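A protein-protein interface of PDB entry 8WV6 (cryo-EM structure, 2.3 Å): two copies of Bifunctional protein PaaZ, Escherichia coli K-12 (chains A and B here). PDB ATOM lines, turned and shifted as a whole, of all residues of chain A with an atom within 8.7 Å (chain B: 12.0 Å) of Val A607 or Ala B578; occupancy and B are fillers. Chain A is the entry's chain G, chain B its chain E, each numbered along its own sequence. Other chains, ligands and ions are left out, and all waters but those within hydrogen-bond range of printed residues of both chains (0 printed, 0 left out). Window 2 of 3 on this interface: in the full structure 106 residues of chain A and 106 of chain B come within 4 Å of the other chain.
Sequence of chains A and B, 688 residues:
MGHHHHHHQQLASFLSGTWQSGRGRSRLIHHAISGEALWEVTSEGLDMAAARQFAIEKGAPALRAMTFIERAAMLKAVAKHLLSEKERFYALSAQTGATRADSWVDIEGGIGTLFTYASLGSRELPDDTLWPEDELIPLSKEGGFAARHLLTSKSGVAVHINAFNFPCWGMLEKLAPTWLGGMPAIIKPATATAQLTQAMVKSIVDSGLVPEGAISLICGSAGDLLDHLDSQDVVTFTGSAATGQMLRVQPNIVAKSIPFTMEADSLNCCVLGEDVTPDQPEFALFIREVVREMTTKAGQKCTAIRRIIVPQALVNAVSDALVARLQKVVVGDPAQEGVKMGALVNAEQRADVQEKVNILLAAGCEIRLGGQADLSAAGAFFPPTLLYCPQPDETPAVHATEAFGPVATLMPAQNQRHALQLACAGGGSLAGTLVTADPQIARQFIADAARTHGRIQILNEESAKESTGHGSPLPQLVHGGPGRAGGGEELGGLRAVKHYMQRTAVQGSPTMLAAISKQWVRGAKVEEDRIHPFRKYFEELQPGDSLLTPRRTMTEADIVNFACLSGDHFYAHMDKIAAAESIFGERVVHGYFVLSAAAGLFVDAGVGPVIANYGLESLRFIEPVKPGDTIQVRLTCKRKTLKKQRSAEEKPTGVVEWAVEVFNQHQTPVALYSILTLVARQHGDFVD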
ATOM      1  N   PHE A 534      -6.560 -27.191   3.895  1.00  0.00           N
ATOM      2  CA  PHE A 534      -7.347 -26.700   5.021  1.00  0.00           C
ATOM      3  C   PHE A 534      -7.861 -27.810   5.927  1.00  0.00           C
ATOM      4  O   PHE A 534      -8.477 -27.505   6.949  1.00  0.00           O
ATOM      5  CB  PHE A 534      -8.544 -25.881   4.538  1.00  0.00           C
ATOM      6  CG  PHE A 534      -8.219 -24.457   4.211  1.00  0.00           C
ATOM      7  CD1 PHE A 534      -6.916 -24.052   4.017  1.00  0.00           C
ATOM      8  CD2 PHE A 534      -9.226 -23.519   4.104  1.00  0.00           C
ATOM      9  CE1 PHE A 534      -6.624 -22.742   3.720  1.00  0.00           C
ATOM     10  CE2 PHE A 534      -8.936 -22.207   3.803  1.00  0.00           C
ATOM     11  CZ  PHE A 534      -7.635 -21.821   3.614  1.00  0.00           C
ATOM     12  N   ARG A 535      -7.641 -29.072   5.584  1.00  0.00           N
ATOM     13  CA  ARG A 535      -8.080 -30.165   6.434  1.00  0.00           C
ATOM     14  C   ARG A 535      -6.972 -30.692   7.327  1.00  0.00           C
ATOM     15  O   ARG A 535      -7.230 -31.557   8.166  1.00  0.00           O
ATOM     16  CB  ARG A 535      -8.647 -31.299   5.582  1.00  0.00           C
ATOM     17  CG  ARG A 535      -9.909 -30.906   4.864  1.00  0.00           C
ATOM     18  CD  ARG A 535     -10.547 -32.062   4.140  1.00  0.00           C
ATOM     19  NE  ARG A 535     -11.636 -31.606   3.286  1.00  0.00           N
ATOM     20  CZ  ARG A 535     -12.432 -32.407   2.587  1.00  0.00           C
ATOM     21  NH1 ARG A 535     -12.267 -33.720   2.637  1.00  0.00           N
ATOM     22  NH2 ARG A 535     -13.395 -31.894   1.840  1.00  0.00           N
ATOM     23  N   TYR A 537      -4.277 -30.456  10.365  1.00  0.00           N
ATOM     24  CA  TYR A 537      -3.971 -29.766  11.602  1.00  0.00           C
ATOM     25  C   TYR A 537      -2.613 -29.088  11.494  1.00  0.00           C
ATOM     26  O   TYR A 537      -1.850 -29.319  10.555  1.00  0.00           O
ATOM     27  CB  TYR A 537      -3.997 -30.731  12.780  1.00  0.00           C
ATOM     28  CG  TYR A 537      -5.385 -31.134  13.169  1.00  0.00           C
ATOM     29  CD1 TYR A 537      -6.032 -32.167  12.513  1.00  0.00           C
ATOM     30  CD2 TYR A 537      -6.064 -30.468  14.173  1.00  0.00           C
ATOM     31  CE1 TYR A 537      -7.301 -32.535  12.856  1.00  0.00           C
ATOM     32  CE2 TYR A 537      -7.339 -30.830  14.524  1.00  0.00           C
ATOM     33  CZ  TYR A 537      -7.953 -31.865  13.861  1.00  0.00           C
ATOM     34  OH  TYR A 537      -9.228 -32.236  14.200  1.00  0.00           O
ATOM     35  N   ASP A 604     -12.026 -24.290   1.914  1.00  0.00           N
ATOM     36  CA  ASP A 604     -12.740 -25.521   2.227  1.00  0.00           C
ATOM     37  C   ASP A 604     -13.925 -25.210   3.135  1.00  0.00           C
ATOM     38  O   ASP A 604     -13.759 -24.605   4.197  1.00  0.00           O
ATOM     39  CB  ASP A 604     -11.801 -26.522   2.897  1.00  0.00           C
ATOM     40  CG  ASP A 604     -12.287 -27.942   2.783  1.00  0.00           C
ATOM     41  OD1 ASP A 604     -12.336 -28.455   1.653  1.00  0.00           O
ATOM     42  OD2 ASP A 604     -12.621 -28.547   3.819  1.00  0.00           O
ATOM     43  N   ALA A 605     -15.114 -25.653   2.730  1.00  0.00           N
ATOM     44  CA  ALA A 605     -16.349 -25.200   3.363  1.00  0.00           C
ATOM     45  C   ALA A 605     -16.587 -25.824   4.735  1.00  0.00           C
ATOM     46  O   ALA A 605     -17.030 -25.136   5.659  1.00  0.00           O
ATOM     47  CB  ALA A 605     -17.539 -25.489   2.450  1.00  0.00           C
ATOM     48  N   GLY A 606     -16.304 -27.112   4.900  1.00  0.00           N
ATOM     49  CA  GLY A 606     -16.728 -27.802   6.097  1.00  0.00           C
ATOM     50  C   GLY A 606     -15.862 -27.502   7.307  1.00  0.00           C
ATOM     51  O   GLY A 606     -14.750 -26.988   7.212  1.00  0.00           O
ATOM     52  N   VAL A 607     -16.402 -27.853   8.473  1.00  0.00           N
ATOM     53  CA  VAL A 607     -15.682 -27.703   9.734  1.00  0.00           C
ATOM     54  C   VAL A 607     -14.357 -28.448   9.665  1.00  0.00           C
ATOM     55  O   VAL A 607     -14.296 -29.610   9.246  1.00  0.00           O
ATOM     56  CB  VAL A 607     -16.542 -28.204  10.903  1.00  0.00           C
ATOM     57  CG1 VAL A 607     -15.702 -28.393  12.142  1.00  0.00           C
ATOM     58  CG2 VAL A 607     -17.659 -27.227  11.183  1.00  0.00           C
ATOM     59  N   GLY A 608     -13.284 -27.774  10.069  1.00  0.00           N
ATOM     60  CA  GLY A 608     -11.969 -28.361  10.075  1.00  0.00           C
ATOM     61  C   GLY A 608     -11.002 -27.591  10.950  1.00  0.00           C
ATOM     62  O   GLY A 608     -11.398 -26.785  11.791  1.00  0.00           O
ATOM     63  N   PRO A 609      -9.704 -27.830  10.765  1.00  0.00           N
ATOM     64  CA  PRO A 609      -8.704 -27.155  11.608  1.00  0.00           C
ATOM     65  C   PRO A 609      -8.633 -25.649  11.422  1.00  0.00           C
ATOM     66  O   PRO A 609      -8.330 -24.942  12.386  1.00  0.00           O
ATOM     67  CB  PRO A 609      -7.391 -27.828  11.197  1.00  0.00           C
ATOM     68  CG  PRO A 609      -7.785 -29.081  10.538  1.00  0.00           C
ATOM     69  CD  PRO A 609      -9.102 -28.864   9.913  1.00  0.00           C
ATOM     70  N   VAL A 610      -8.898 -25.128  10.223  1.00  0.00           N
ATOM     71  CA  VAL A 610      -8.803 -23.691  10.007  1.00  0.00           C
ATOM     72  C   VAL A 610      -9.910 -22.987  10.777  1.00  0.00           C
ATOM     73  O   VAL A 610     -11.098 -23.258  10.574  1.00  0.00           O
ATOM     74  CB  VAL A 610      -8.863 -23.361   8.510  1.00  0.00           C
ATOM     75  CG1 VAL A 610      -9.017 -21.863   8.313  1.00  0.00           C
ATOM     76  CG2 VAL A 610      -7.615 -23.859   7.814  1.00  0.00           C
ATOM     77  N   ILE A 611      -9.522 -22.059  11.647  1.00  0.00           N
ATOM     78  CA  ILE A 611     -10.444 -21.440  12.592  1.00  0.00           C
ATOM     79  C   ILE A 611     -10.830 -20.039  12.139  1.00  0.00           C
ATOM     80  O   ILE A 611     -12.012 -19.682  12.146  1.00  0.00           O
ATOM     81  CB  ILE A 611      -9.827 -21.414  14.001  1.00  0.00           C
ATOM     82  CG1 ILE A 611      -9.802 -22.817  14.598  1.00  0.00           C
ATOM     83  CG2 ILE A 611     -10.582 -20.478  14.900  1.00  0.00           C
ATOM     84  CD1 ILE A 611      -8.904 -22.928  15.793  1.00  0.00           C
ATOM     85  N   ASP B 568     -17.758 -18.665  -1.617  1.00  0.00           N
ATOM     86  CA  ASP B 568     -17.181 -18.998  -0.318  1.00  0.00           C
ATOM     87  C   ASP B 568     -18.295 -19.370   0.652  1.00  0.00           C
ATOM     88  O   ASP B 568     -18.931 -18.493   1.237  1.00  0.00           O
ATOM     89  CB  ASP B 568     -16.356 -17.833   0.222  1.00  0.00           C
ATOM     90  CG  ASP B 568     -15.750 -18.121   1.587  1.00  0.00           C
ATOM     91  OD1 ASP B 568     -15.848 -19.260   2.071  1.00  0.00           O
ATOM     92  OD2 ASP B 568     -15.159 -17.199   2.181  1.00  0.00           O
ATOM     93  N   HIS B 569     -18.492 -20.670   0.857  1.00  0.00           N
ATOM     94  CA  HIS B 569     -19.523 -21.193   1.744  1.00  0.00           C
ATOM     95  C   HIS B 569     -18.931 -21.718   3.046  1.00  0.00           C
ATOM     96  O   HIS B 569     -19.386 -22.717   3.598  1.00  0.00           O
ATOM     97  CB  HIS B 569     -20.331 -22.278   1.041  1.00  0.00           C
ATOM     98  CG  HIS B 569     -20.999 -21.801  -0.209  1.00  0.00           C
ATOM     99  ND1 HIS B 569     -22.138 -21.031  -0.195  1.00  0.00           N
ATOM    100  CD2 HIS B 569     -20.669 -21.960  -1.511  1.00  0.00           C
ATOM    101  CE1 HIS B 569     -22.489 -20.745  -1.435  1.00  0.00           C
ATOM    102  NE2 HIS B 569     -21.614 -21.298  -2.252  1.00  0.00           N
ATOM    103  N   PHE B 570     -17.902 -21.042   3.541  1.00  0.00           N
ATOM    104  CA  PHE B 570     -17.299 -21.382   4.823  1.00  0.00           C
ATOM    105  C   PHE B 570     -18.347 -21.417   5.931  1.00  0.00           C
ATOM    106  O   PHE B 570     -19.231 -20.561   5.998  1.00  0.00           O
ATOM    107  CB  PHE B 570     -16.211 -20.365   5.144  1.00  0.00           C
ATOM    108  CG  PHE B 570     -15.363 -20.731   6.308  1.00  0.00           C
ATOM    109  CD1 PHE B 570     -14.472 -21.782   6.224  1.00  0.00           C
ATOM    110  CD2 PHE B 570     -15.440 -20.017   7.482  1.00  0.00           C
ATOM    111  CE1 PHE B 570     -13.678 -22.113   7.290  1.00  0.00           C
ATOM    112  CE2 PHE B 570     -14.652 -20.344   8.548  1.00  0.00           C
ATOM    113  CZ  PHE B 570     -13.767 -21.397   8.455  1.00  0.00           C
ATOM    114  N   TYR B 571     -18.238 -22.416   6.815  1.00  0.00           N
ATOM    115  CA  TYR B 571     -19.322 -22.707   7.754  1.00  0.00           C
ATOM    116  C   TYR B 571     -19.631 -21.542   8.682  1.00  0.00           C
ATOM    117  O   TYR B 571     -20.755 -21.439   9.176  1.00  0.00           O
ATOM    118  CB  TYR B 571     -19.003 -23.946   8.589  1.00  0.00           C
ATOM    119  CG  TYR B 571     -17.807 -23.793   9.490  1.00  0.00           C
ATOM    120  CD1 TYR B 571     -16.543 -24.093   9.028  1.00  0.00           C
ATOM    121  CD2 TYR B 571     -17.939 -23.342  10.799  1.00  0.00           C
ATOM    122  CE1 TYR B 571     -15.448 -23.964   9.829  1.00  0.00           C
ATOM    123  CE2 TYR B 571     -16.838 -23.209  11.615  1.00  0.00           C
ATOM    124  CZ  TYR B 571     -15.594 -23.520  11.117  1.00  0.00           C
ATOM    125  OH  TYR B 571     -14.477 -23.400  11.900  1.00  0.00           O
ATOM    126  N   ALA B 572     -18.664 -20.663   8.944  1.00  0.00           N
ATOM    127  CA  ALA B 572     -18.943 -19.546   9.838  1.00  0.00           C
ATOM    128  C   ALA B 572     -19.953 -18.566   9.257  1.00  0.00           C
ATOM    129  O   ALA B 572     -20.436 -17.694   9.983  1.00  0.00           O
ATOM    130  CB  ALA B 572     -17.649 -18.815  10.193  1.00  0.00           C
ATOM    131  N   HIS B 573     -20.292 -18.697   7.985  1.00  0.00           N
ATOM    132  CA  HIS B 573     -21.260 -17.840   7.327  1.00  0.00           C
ATOM    133  C   HIS B 573     -22.530 -18.558   6.916  1.00  0.00           C
ATOM    134  O   HIS B 573     -23.591 -17.941   6.936  1.00  0.00           O
ATOM    135  CB  HIS B 573     -20.630 -17.199   6.085  1.00  0.00           C
ATOM    136  CG  HIS B 573     -19.262 -16.651   6.327  1.00  0.00           C
ATOM    137  ND1 HIS B 573     -18.161 -17.033   5.592  1.00  0.00           N
ATOM    138  CD2 HIS B 573     -18.813 -15.762   7.240  1.00  0.00           C
ATOM    139  CE1 HIS B 573     -17.096 -16.397   6.039  1.00  0.00           C
ATOM    140  NE2 HIS B 573     -17.465 -15.616   7.036  1.00  0.00           N
ATOM    141  N   MET B 574     -22.457 -19.842   6.559  1.00  0.00           N
ATOM    142  CA  MET B 574     -23.560 -20.538   5.913  1.00  0.00           C
ATOM    143  C   MET B 574     -24.166 -21.679   6.720  1.00  0.00           C
ATOM    144  O   MET B 574     -25.157 -22.261   6.270  1.00  0.00           O
ATOM    145  CB  MET B 574     -23.105 -21.086   4.550  1.00  0.00           C
ATOM    146  CG  MET B 574     -22.866 -20.017   3.494  1.00  0.00           C
ATOM    147  SD  MET B 574     -24.297 -18.954   3.212  1.00  0.00           S
ATOM    148  CE  MET B 574     -25.075 -19.787   1.827  1.00  0.00           C
ATOM    149  N   ASP B 575     -23.618 -22.020   7.883  1.00  0.00           N
ATOM    150  CA  ASP B 575     -24.040 -23.191   8.649  1.00  0.00           C
ATOM    151  C   ASP B 575     -24.303 -22.748  10.081  1.00  0.00           C
ATOM    152  O   ASP B 575     -23.365 -22.546  10.855  1.00  0.00           O
ATOM    153  CB  ASP B 575     -22.975 -24.285   8.585  1.00  0.00           C
ATOM    154  CG  ASP B 575     -23.327 -25.520   9.405  1.00  0.00           C
ATOM    155  OD1 ASP B 575     -24.460 -25.646   9.906  1.00  0.00           O
ATOM    156  OD2 ASP B 575     -22.452 -26.391   9.535  1.00  0.00           O
ATOM    157  N   LYS B 576     -25.579 -22.626  10.438  1.00  0.00           N
ATOM    158  CA  LYS B 576     -25.947 -22.105  11.750  1.00  0.00           C
ATOM    159  C   LYS B 576     -25.554 -23.068  12.870  1.00  0.00           C
ATOM    160  O   LYS B 576     -25.187 -22.634  13.967  1.00  0.00           O
ATOM    161  CB  LYS B 576     -27.444 -21.806  11.762  1.00  0.00           C
ATOM    162  CG  LYS B 576     -28.003 -21.340  13.071  1.00  0.00           C
ATOM    163  CD  LYS B 576     -29.237 -20.500  12.848  1.00  0.00           C
ATOM    164  CE  LYS B 576     -30.385 -21.314  12.304  1.00  0.00           C
ATOM    165  NZ  LYS B 576     -31.593 -20.454  12.192  1.00  0.00           N
ATOM    166  N   ILE B 577     -25.571 -24.374  12.593  1.00  0.00           N
ATOM    167  CA  ILE B 577     -25.249 -25.367  13.615  1.00  0.00           C
ATOM    168  C   ILE B 577     -23.764 -25.331  13.955  1.00  0.00           C
ATOM    169  O   ILE B 577     -23.382 -25.318  15.129  1.00  0.00           O
ATOM    170  CB  ILE B 577     -25.684 -26.769  13.156  1.00  0.00           C
ATOM    171  CG1 ILE B 577     -27.202 -26.869  13.152  1.00  0.00           C
ATOM    172  CG2 ILE B 577     -25.086 -27.843  14.056  1.00  0.00           C
ATOM    173  CD1 ILE B 577     -27.720 -27.691  12.044  1.00  0.00           C
ATOM    174  N   ALA B 578     -22.902 -25.330  12.939  1.00  0.00           N
ATOM    175  CA  ALA B 578     -21.470 -25.258  13.209  1.00  0.00           C
ATOM    176  C   ALA B 578     -21.077 -23.898  13.765  1.00  0.00           C
ATOM    177  O   ALA B 578     -20.189 -23.808  14.618  1.00  0.00           O
ATOM    178  CB  ALA B 578     -20.671 -25.565  11.948  1.00  0.00           C
ATOM    179  N   ALA B 579     -21.729 -22.829  13.305  1.00  0.00           N
ATOM    180  CA  ALA B 579     -21.427 -21.504  13.829  1.00  0.00           C
ATOM    181  C   ALA B 579     -21.859 -21.364  15.279  1.00  0.00           C
ATOM    182  O   ALA B 579     -21.291 -20.550  16.009  1.00  0.00           O
ATOM    183  CB  ALA B 579     -22.092 -20.422  12.981  1.00  0.00           C
ATOM    184  N   ALA B 580     -22.862 -22.137  15.709  1.00  0.00           N
ATOM    185  CA  ALA B 580     -23.275 -22.103  17.107  1.00  0.00           C
ATOM    186  C   ALA B 580     -22.124 -22.426  18.052  1.00  0.00           C
ATOM    187  O   ALA B 580     -21.989 -21.781  19.095  1.00  0.00           O
ATOM    188  CB  ALA B 580     -24.435 -23.066  17.344  1.00  0.00           C
ATOM    189  N   GLU B 581     -21.294 -23.416  17.728  1.00  0.00           N
ATOM    190  CA  GLU B 581     -20.120 -23.687  18.547  1.00  0.00           C
ATOM    191  C   GLU B 581     -18.837 -23.098  17.978  1.00  0.00           C
ATOM    192  O   GLU B 581     -17.760 -23.642  18.230  1.00  0.00           O
ATOM    193  CB  GLU B 581     -19.933 -25.191  18.793  1.00  0.00           C
ATOM    194  CG  GLU B 581     -19.597 -26.056  17.600  1.00  0.00           C
ATOM    195  CD  GLU B 581     -20.824 -26.646  16.958  1.00  0.00           C
ATOM    196  OE1 GLU B 581     -21.936 -26.172  17.260  1.00  0.00           O
ATOM    197  OE2 GLU B 581     -20.680 -27.597  16.163  1.00  0.00           O
ATOM    198  N   SER B 582     -18.917 -22.001  17.239  1.00  0.00           N
ATOM    199  CA  SER B 582     -17.714 -21.256  16.913  1.00  0.00           C
ATOM    200  C   SER B 582     -17.403 -20.274  18.041  1.00  0.00           C
ATOM    201  O   SER B 582     -18.113 -20.191  19.045  1.00  0.00           O
ATOM    202  CB  SER B 582     -17.876 -20.549  15.572  1.00  0.00           C
ATOM    203  OG  SER B 582     -18.581 -19.330  15.713  1.00  0.00           O
ATOM    204  N   ILE B 583     -16.318 -19.517  17.878  1.00  0.00           N
ATOM    205  CA  ILE B 583     -15.973 -18.509  18.875  1.00  0.00           C
ATOM    206  C   ILE B 583     -17.006 -17.391  18.875  1.00  0.00           C
ATOM    207  O   ILE B 583     -17.340 -16.831  19.927  1.00  0.00           O
ATOM    208  CB  ILE B 583     -14.556 -17.962  18.627  1.00  0.00           C
ATOM    209  CG1 ILE B 583     -13.512 -19.071  18.743  1.00  0.00           C
ATOM    210  CG2 ILE B 583     -14.234 -16.855  19.614  1.00  0.00           C
ATOM    211  CD1 ILE B 583     -13.213 -19.781  17.442  1.00  0.00           C
ATOM    212  N   PHE B 584     -17.542 -17.059  17.699  1.00  0.00           N
ATOM    213  CA  PHE B 584     -18.508 -15.973  17.602  1.00  0.00           C
ATOM    214  C   PHE B 584     -19.868 -16.388  18.149  1.00  0.00           C
ATOM    215  O   PHE B 584     -20.568 -15.580  18.769  1.00  0.00           O
ATOM    216  CB  PHE B 584     -18.621 -15.513  16.150  1.00  0.00           C
ATOM    217  CG  PHE B 584     -17.328 -14.993  15.575  1.00  0.00           C
ATOM    218  CD1 PHE B 584     -16.511 -14.158  16.316  1.00  0.00           C
ATOM    219  CD2 PHE B 584     -16.933 -15.341  14.293  1.00  0.00           C
ATOM    220  CE1 PHE B 584     -15.317 -13.681  15.789  1.00  0.00           C
ATOM    221  CE2 PHE B 584     -15.751 -14.865  13.758  1.00  0.00           C
ATOM    222  CZ  PHE B 584     -14.940 -14.035  14.505  1.00  0.00           C
ATOM    223  N   GLY B 585     -20.264 -17.637  17.929  1.00  0.00           N
ATOM    224  CA  GLY B 585     -21.512 -18.147  18.447  1.00  0.00           C
ATOM    225  C   GLY B 585     -22.705 -17.987  17.531  1.00  0.00           C
ATOM    226  O   GLY B 585     -23.804 -18.408  17.900  1.00  0.00           O
ATOM    227  N   GLU B 586     -22.525 -17.377  16.365  1.00  0.00           N
ATOM    228  CA  GLU B 586     -23.571 -17.289  15.356  1.00  0.00           C
ATOM    229  C   GLU B 586     -22.909 -16.960  14.026  1.00  0.00           C
ATOM    230  O   GLU B 586     -21.693 -16.780  13.948  1.00  0.00           O
ATOM    231  CB  GLU B 586     -24.639 -16.256  15.728  1.00  0.00           C
ATOM    232  CG  GLU B 586     -24.134 -14.845  15.943  1.00  0.00           C
ATOM    233  CD  GLU B 586     -25.243 -13.898  16.376  1.00  0.00           C
ATOM    234  OE1 GLU B 586     -26.407 -14.340  16.473  1.00  0.00           O
ATOM    235  OE2 GLU B 586     -24.961 -12.716  16.633  1.00  0.00           O
ATOM    236  N   ARG B 587     -23.718 -16.916  12.973  1.00  0.00           N
ATOM    237  CA  ARG B 587     -23.201 -16.610  11.648  1.00  0.00           C
ATOM    238  C   ARG B 587     -22.775 -15.153  11.550  1.00  0.00           C
ATOM    239  O   ARG B 587     -23.464 -14.254  12.035  1.00  0.00           O
ATOM    240  CB  ARG B 587     -24.248 -16.918  10.585  1.00  0.00           C
ATOM    241  CG  ARG B 587     -24.295 -18.367  10.159  1.00  0.00           C
ATOM    242  CD  ARG B 587     -25.562 -18.635   9.407  1.00  0.00           C
ATOM    243  NE  ARG B 587     -26.742 -18.294  10.192  1.00  0.00           N
ATOM    244  CZ  ARG B 587     -27.893 -17.904   9.662  1.00  0.00           C
ATOM    245  NH1 ARG B 587     -28.012 -17.801   8.350  1.00  0.00           N
ATOM    246  NH2 ARG B 587     -28.926 -17.618  10.440  1.00  0.00           N
ATOM    247  N   VAL B 588     -21.622 -14.923  10.923  1.00  0.00           N
ATOM    248  CA  VAL B 588     -21.105 -13.572  10.723  1.00  0.00           C
ATOM    249  C   VAL B 588     -20.995 -13.254   9.234  1.00  0.00           C
ATOM    250  O   VAL B 588     -21.217 -14.115   8.380  1.00  0.00           O
ATOM    251  CB  VAL B 588     -19.748 -13.382  11.425  1.00  0.00           C
ATOM    252  CG1 VAL B 588     -19.857 -13.719  12.895  1.00  0.00           C
ATOM    253  CG2 VAL B 588     -18.671 -14.219  10.763  1.00  0.00           C
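The backbone NH (N) of Tyr B571 is in hydrogen-bond range of the backbone carbonyl oxygen (O) of Ala A605, 3.2 Å away.
The backbone NH (N) of Phe B570 sits at hydrogen-bond distance from the side-chain carboxylate (OD1) of Asp B568, 3.1 Å away. The side-chain carboxylate (OD1) of Asp B575 is in hydrogen-bond range of the backbone NH (N) of Ala B578, 3.4 Å away. The side-chain carboxylate (OD2) of Asp A604 lies within salt-bridge range of the guanidinium group (NE) of Arg A535 (3.3 Å).
Among the printed residues, pairs that only touch across the chains: Ala A605 with His B569 (3.5 Å), Val A607 with Ala B578 (3.5 Å), Asp A604 with Phe B570 (3.5 Å), Val A610 with Tyr B571 (3.6 Å), Ile A611 with Ile B583 (3.7 Å), Val A607 with Tyr B571 (3.7 Å), Ala A605 with Phe B570 (3.9 Å), Gly A606 with Tyr B571 (3.9 Å) and Val A610 with Phe B570 (3.9 Å).
Of the printed residues of chain B, Asp A604 touches Phe B570. Val A607 touches just these residues of chain B: Tyr B571 (3.7 Å) and Ala B578 (3.5 Å). No residue of chain B comes within 4 Å of Pro A609. Printed residues of chain B within 4 Å of Ile A611: Ile B583. Printed residues of chain A within 4 Å of His B569: Ala A605. Of the printed residues of chain A, Phe B570 touches Asp A604, Ala A605 and Val A610. Of the printed residues of chain A, Tyr B571 touches Ala A605, Gly A606, Val A607 and Val A610. No residue of chain A comes within 4 Å of Ala B579. No residue of chain A comes within 4 Å of Glu B581. Gly B585 touches none of the printed residues of chain A. The nearest residue of chain A that does not touch Ala B578 is Gly A606 (7.0 Å).
Printed residues of chain A that touch a printed residue of chain B: Asp A604, Ala A605, Gly A606, Val A607, Val A610 and Ile A611. Along chain A the printed residues that touch a printed residue of chain B span positions 604 to 611. Of the 21 printed residues of chain B, 5 touch a printed residue of chain A. Printed residues of chain B that touch a printed residue of chain A: His B569, Phe B570, Tyr B571, Ala B578 and Ile B583. Hydrophobic or aromatic side chains of chain B that line the printed part of chain A: Phe B570, Tyr B571, Ala B578 and Ile B583. Among the printed residues, 10 pairs touch across the chains.
No position is printed for both chains.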
